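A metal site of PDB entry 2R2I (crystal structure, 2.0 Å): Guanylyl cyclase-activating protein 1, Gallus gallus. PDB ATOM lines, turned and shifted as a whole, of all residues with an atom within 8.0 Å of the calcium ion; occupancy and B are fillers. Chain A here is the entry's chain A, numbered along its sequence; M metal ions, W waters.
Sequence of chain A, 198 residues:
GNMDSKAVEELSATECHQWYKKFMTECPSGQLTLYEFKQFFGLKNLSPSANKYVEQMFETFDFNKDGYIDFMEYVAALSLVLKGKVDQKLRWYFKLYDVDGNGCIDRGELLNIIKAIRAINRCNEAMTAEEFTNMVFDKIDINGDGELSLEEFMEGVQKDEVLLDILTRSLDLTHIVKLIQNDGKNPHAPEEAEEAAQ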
ATOM      1  N   GLN A  31      17.738  10.382  16.719  1.00  0.00           N
ATOM      2  CA  GLN A  31      18.810   9.387  16.632  1.00  0.00           C
ATOM      3  C   GLN A  31      18.300   7.977  16.842  1.00  0.00           C
ATOM      4  O   GLN A  31      17.287   7.749  17.505  1.00  0.00           O
ATOM      5  CB  GLN A  31      19.874   9.634  17.702  1.00  0.00           C
ATOM      6  CG  GLN A  31      20.492  11.006  17.729  1.00  0.00           C
ATOM      7  CD  GLN A  31      21.508  11.119  18.853  1.00  0.00           C
ATOM      8  OE1 GLN A  31      21.181  10.876  20.018  1.00  0.00           O
ATOM      9  NE2 GLN A  31      22.742  11.475  18.507  1.00  0.00           N
ATOM     10  N   LEU A  32      19.036   7.013  16.291  1.00  0.00           N
ATOM     11  CA  LEU A  32      18.724   5.601  16.445  1.00  0.00           C
ATOM     12  C   LEU A  32      19.998   4.858  16.849  1.00  0.00           C
ATOM     13  O   LEU A  32      21.041   5.004  16.190  1.00  0.00           O
ATOM     14  CB  LEU A  32      18.219   5.005  15.124  1.00  0.00           C
ATOM     15  CG  LEU A  32      16.780   5.201  14.641  1.00  0.00           C
ATOM     16  CD1 LEU A  32      16.719   5.122  13.126  1.00  0.00           C
ATOM     17  CD2 LEU A  32      15.895   4.135  15.259  1.00  0.00           C
ATOM     18  N   PHE A  58      24.483  -0.967   9.766  1.00  0.00           N
ATOM     19  CA  PHE A  58      24.274   0.154  10.669  1.00  0.00           C
ATOM     20  C   PHE A  58      25.554   0.985  10.750  1.00  0.00           C
ATOM     21  O   PHE A  58      25.547   2.204  10.594  1.00  0.00           O
ATOM     22  CB  PHE A  58      23.914  -0.362  12.077  1.00  0.00           C
ATOM     23  CG  PHE A  58      23.728   0.739  13.104  1.00  0.00           C
ATOM     24  CD1 PHE A  58      22.493   1.375  13.265  1.00  0.00           C
ATOM     25  CD2 PHE A  58      24.787   1.151  13.910  1.00  0.00           C
ATOM     26  CE1 PHE A  58      22.318   2.397  14.206  1.00  0.00           C
ATOM     27  CE2 PHE A  58      24.622   2.171  14.860  1.00  0.00           C
ATOM     28  CZ  PHE A  58      23.392   2.793  15.013  1.00  0.00           C
ATOM     29  N   GLU A  59      26.681   0.314  10.991  1.00  0.00           N
ATOM     30  CA  GLU A  59      27.955   0.994  11.099  1.00  0.00           C
ATOM     31  C   GLU A  59      28.299   1.730   9.809  1.00  0.00           C
ATOM     32  O   GLU A  59      28.854   2.830   9.837  1.00  0.00           O
ATOM     33  CB  GLU A  59      29.060  -0.010  11.441  1.00  0.00           C
ATOM     34  CG  GLU A  59      28.751  -0.859  12.656  1.00  0.00           C
ATOM     35  CD  GLU A  59      29.930  -1.714  13.082  1.00  0.00           C
ATOM     36  OE1 GLU A  59      30.580  -2.306  12.193  1.00  0.00           O
ATOM     37  OE2 GLU A  59      30.197  -1.805  14.299  1.00  0.00           O
ATOM     38  N   PHE A  61      26.234   3.082   7.691  1.00  0.00           N
ATOM     39  CA  PHE A  61      25.418   4.291   7.604  1.00  0.00           C
ATOM     40  C   PHE A  61      25.695   5.283   8.743  1.00  0.00           C
ATOM     41  O   PHE A  61      25.274   6.446   8.698  1.00  0.00           O
ATOM     42  CB  PHE A  61      23.934   3.915   7.561  1.00  0.00           C
ATOM     43  CG  PHE A  61      23.552   3.142   6.325  1.00  0.00           C
ATOM     44  CD1 PHE A  61      22.728   2.026   6.411  1.00  0.00           C
ATOM     45  CD2 PHE A  61      24.014   3.528   5.063  1.00  0.00           C
ATOM     46  CE1 PHE A  61      22.367   1.301   5.265  1.00  0.00           C
ATOM     47  CE2 PHE A  61      23.654   2.817   3.919  1.00  0.00           C
ATOM     48  CZ  PHE A  61      22.832   1.699   4.022  1.00  0.00           C
ATOM     49  N   ASP A  62      26.410   4.830   9.768  1.00  0.00           N
ATOM     50  CA  ASP A  62      26.789   5.698  10.884  1.00  0.00           C
ATOM     51  C   ASP A  62      28.043   6.420  10.406  1.00  0.00           C
ATOM     52  O   ASP A  62      29.156   6.075  10.793  1.00  0.00           O
ATOM     53  CB  ASP A  62      27.124   4.870  12.135  1.00  0.00           C
ATOM     54  CG  ASP A  62      27.597   5.716  13.304  1.00  0.00           C
ATOM     55  OD1 ASP A  62      28.014   5.146  14.331  1.00  0.00           O
ATOM     56  OD2 ASP A  62      27.530   6.965  13.214  1.00  0.00           O
ATOM     57  N   PHE A  63      27.844   7.416   9.555  1.00  0.00           N
ATOM     58  CA  PHE A  63      28.940   8.179   8.960  1.00  0.00           C
ATOM     59  C   PHE A  63      29.976   8.716   9.923  1.00  0.00           C
ATOM     60  O   PHE A  63      31.174   8.553   9.696  1.00  0.00           O
ATOM     61  CB  PHE A  63      28.375   9.322   8.107  1.00  0.00           C
ATOM     62  CG  PHE A  63      27.562   8.856   6.926  1.00  0.00           C
ATOM     63  CD1 PHE A  63      26.712   9.736   6.278  1.00  0.00           C
ATOM     64  CD2 PHE A  63      27.656   7.541   6.465  1.00  0.00           C
ATOM     65  CE1 PHE A  63      25.955   9.307   5.179  1.00  0.00           C
ATOM     66  CE2 PHE A  63      26.905   7.103   5.388  1.00  0.00           C
ATOM     67  CZ  PHE A  63      26.057   7.997   4.740  1.00  0.00           C
ATOM     68  N   ASN A  64      29.549   9.369  11.004  1.00  0.00           N
ATOM     69  CA  ASN A  64      30.518   9.908  11.943  1.00  0.00           C
ATOM     70  C   ASN A  64      30.926   8.913  13.030  1.00  0.00           C
ATOM     71  O   ASN A  64      31.600   9.284  13.990  1.00  0.00           O
ATOM     72  CB  ASN A  64      30.002  11.214  12.562  1.00  0.00           C
ATOM     73  CG  ASN A  64      28.837  11.001  13.511  1.00  0.00           C
ATOM     74  OD1 ASN A  64      28.431   9.870  13.761  1.00  0.00           O
ATOM     75  ND2 ASN A  64      28.310  12.101  14.041  1.00  0.00           N
ATOM     76  N   LYS A  65      30.528   7.657  12.867  1.00  0.00           N
ATOM     77  CA  LYS A  65      30.891   6.606  13.827  1.00  0.00           C
ATOM     78  C   LYS A  65      30.683   6.938  15.305  1.00  0.00           C
ATOM     79  O   LYS A  65      31.525   6.580  16.130  1.00  0.00           O
ATOM     80  CB  LYS A  65      32.346   6.193  13.610  1.00  0.00           C
ATOM     81  CG  LYS A  65      32.534   5.021  12.658  1.00  0.00           C
ATOM     82  CD  LYS A  65      31.972   5.341  11.295  1.00  0.00           C
ATOM     83  CE  LYS A  65      31.893   4.082  10.462  1.00  0.00           C
ATOM     84  NZ  LYS A  65      31.263   4.362   9.159  1.00  0.00           N
ATOM     85  N   ASP A  66      29.596   7.607  15.657  1.00  0.00           N
ATOM     86  CA  ASP A  66      29.362   7.927  17.067  1.00  0.00           C
ATOM     87  C   ASP A  66      28.440   6.904  17.731  1.00  0.00           C
ATOM     88  O   ASP A  66      28.102   7.032  18.917  1.00  0.00           O
ATOM     89  CB  ASP A  66      28.801   9.345  17.229  1.00  0.00           C
ATOM     90  CG  ASP A  66      27.442   9.525  16.572  1.00  0.00           C
ATOM     91  OD1 ASP A  66      26.832  10.603  16.779  1.00  0.00           O
ATOM     92  OD2 ASP A  66      26.990   8.618  15.864  1.00  0.00           O
ATOM     93  N   GLY A  67      28.034   5.888  16.988  1.00  0.00           N
ATOM     94  CA  GLY A  67      27.165   4.874  17.550  1.00  0.00           C
ATOM     95  C   GLY A  67      25.685   5.110  17.336  1.00  0.00           C
ATOM     96  O   GLY A  67      24.861   4.315  17.794  1.00  0.00           O
ATOM     97  N   TYR A  68      25.332   6.195  16.654  1.00  0.00           N
ATOM     98  CA  TYR A  68      23.936   6.515  16.353  1.00  0.00           C
ATOM     99  C   TYR A  68      23.806   6.889  14.882  1.00  0.00           C
ATOM    100  O   TYR A  68      24.774   7.306  14.239  1.00  0.00           O
ATOM    101  CB  TYR A  68      23.437   7.726  17.148  1.00  0.00           C
ATOM    102  CG  TYR A  68      23.600   7.646  18.642  1.00  0.00           C
ATOM    103  CD1 TYR A  68      22.611   7.097  19.452  1.00  0.00           C
ATOM    104  CD2 TYR A  68      24.750   8.149  19.253  1.00  0.00           C
ATOM    105  CE1 TYR A  68      22.764   7.047  20.850  1.00  0.00           C
ATOM    106  CE2 TYR A  68      24.905   8.107  20.640  1.00  0.00           C
ATOM    107  CZ  TYR A  68      23.921   7.559  21.426  1.00  0.00           C
ATOM    108  OH  TYR A  68      24.102   7.509  22.796  1.00  0.00           O
ATOM    109  N   ILE A  69      22.600   6.750  14.345  1.00  0.00           N
ATOM    110  CA  ILE A  69      22.321   7.168  12.980  1.00  0.00           C
ATOM    111  C   ILE A  69      21.391   8.342  13.232  1.00  0.00           C
ATOM    112  O   ILE A  69      20.249   8.146  13.667  1.00  0.00           O
ATOM    113  CB  ILE A  69      21.603   6.093  12.153  1.00  0.00           C
ATOM    114  CG1 ILE A  69      22.607   5.010  11.745  1.00  0.00           C
ATOM    115  CG2 ILE A  69      20.951   6.713  10.917  1.00  0.00           C
ATOM    116  CD1 ILE A  69      22.007   3.879  10.910  1.00  0.00           C
ATOM    117  N   ASP A  70      21.878   9.561  13.018  1.00  0.00           N
ATOM    118  CA  ASP A  70      21.049  10.732  13.259  1.00  0.00           C
ATOM    119  C   ASP A  70      20.213  11.121  12.030  1.00  0.00           C
ATOM    120  O   ASP A  70      20.298  10.475  10.988  1.00  0.00           O
ATOM    121  CB  ASP A  70      21.902  11.910  13.780  1.00  0.00           C
ATOM    122  CG  ASP A  70      22.931  12.390  12.786  1.00  0.00           C
ATOM    123  OD1 ASP A  70      23.967  12.927  13.225  1.00  0.00           O
ATOM    124  OD2 ASP A  70      22.710  12.227  11.566  1.00  0.00           O
ATOM    125  N   PHE A  71      19.389  12.156  12.180  1.00  0.00           N
ATOM    126  CA  PHE A  71      18.494  12.581  11.118  1.00  0.00           C
ATOM    127  C   PHE A  71      19.149  12.825   9.757  1.00  0.00           C
ATOM    128  O   PHE A  71      18.543  12.560   8.720  1.00  0.00           O
ATOM    129  CB  PHE A  71      17.683  13.804  11.572  1.00  0.00           C
ATOM    130  CG  PHE A  71      18.488  15.068  11.704  1.00  0.00           C
ATOM    131  CD1 PHE A  71      18.469  16.021  10.695  1.00  0.00           C
ATOM    132  CD2 PHE A  71      19.245  15.308  12.848  1.00  0.00           C
ATOM    133  CE1 PHE A  71      19.198  17.210  10.808  1.00  0.00           C
ATOM    134  CE2 PHE A  71      19.983  16.494  12.972  1.00  0.00           C
ATOM    135  CZ  PHE A  71      19.958  17.441  11.957  1.00  0.00           C
ATOM    136  N   GLU A  73      22.151  11.411   8.698  1.00  0.00           N
ATOM    137  CA  GLU A  73      22.686  10.150   8.209  1.00  0.00           C
ATOM    138  C   GLU A  73      21.527   9.264   7.755  1.00  0.00           C
ATOM    139  O   GLU A  73      21.670   8.428   6.862  1.00  0.00           O
ATOM    140  CB  GLU A  73      23.479   9.447   9.319  1.00  0.00           C
ATOM    141  CG  GLU A  73      24.607  10.307   9.869  1.00  0.00           C
ATOM    142  CD  GLU A  73      25.240   9.731  11.113  1.00  0.00           C
ATOM    143  OE1 GLU A  73      24.504   9.126  11.923  1.00  0.00           O
ATOM    144  OE2 GLU A  73      26.471   9.911  11.291  1.00  0.00           O
ATOM    145  N   TYR A  74      20.365   9.455   8.384  1.00  0.00           N
ATOM    146  CA  TYR A  74      19.176   8.684   8.053  1.00  0.00           C
ATOM    147  C   TYR A  74      18.742   8.976   6.607  1.00  0.00           C
ATOM    148  O   TYR A  74      18.582   8.058   5.809  1.00  0.00           O
ATOM    149  CB  TYR A  74      18.048   9.044   9.022  1.00  0.00           C
ATOM    150  CG  TYR A  74      16.763   8.255   8.864  1.00  0.00           C
ATOM    151  CD1 TYR A  74      16.656   6.944   9.347  1.00  0.00           C
ATOM    152  CD2 TYR A  74      15.646   8.831   8.282  1.00  0.00           C
ATOM    153  CE1 TYR A  74      15.440   6.242   9.256  1.00  0.00           C
ATOM    154  CE2 TYR A  74      14.432   8.143   8.192  1.00  0.00           C
ATOM    155  CZ  TYR A  74      14.339   6.851   8.675  1.00  0.00           C
ATOM    156  OH  TYR A  74      13.135   6.198   8.593  1.00  0.00           O
HETATM  157 CA    CA M   1      26.237   8.901  13.618  1.00  0.00          CA
HETATM  158  O   HOH W   1      25.216  10.798  14.579  1.00  0.00           O
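The side-chain amino group of Lys 65 lies close to the backbone carbonyl oxygen of Asp 62 (3.2 Å). The backbone NH (N) of Gly 67 is in hydrogen-bond range of the side-chain carboxylate (OD1) of Asp 62. OD2 of Asp 70 is in hydrogen-bond range of N of Glu 73 (3.0 Å). N of Phe 63 lies close to OE2 of Glu 73 (3.3 Å).
Within 4 Å of the calcium ion: Asp 62, Asn 64, Asp 66, Tyr 68 and Glu 73. Along chain A the residues within 4 Å of the calcium ion span positions 62 to 73. The nearest printed residue that does not touch the calcium ion is Ile 69 (4.3 Å).
The calcium ion is bound by O of Tyr 68, water W1, OD2 of Asp 62, OD2 of Asp 66, OD1 of Asn 64, OE1 of Glu 73 and OE2 of Glu 73.
Water W1 lies within hydrogen-bond range of OD1 of Asp 66, OD1 of Asp 70 and ND2 of Asn 64.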
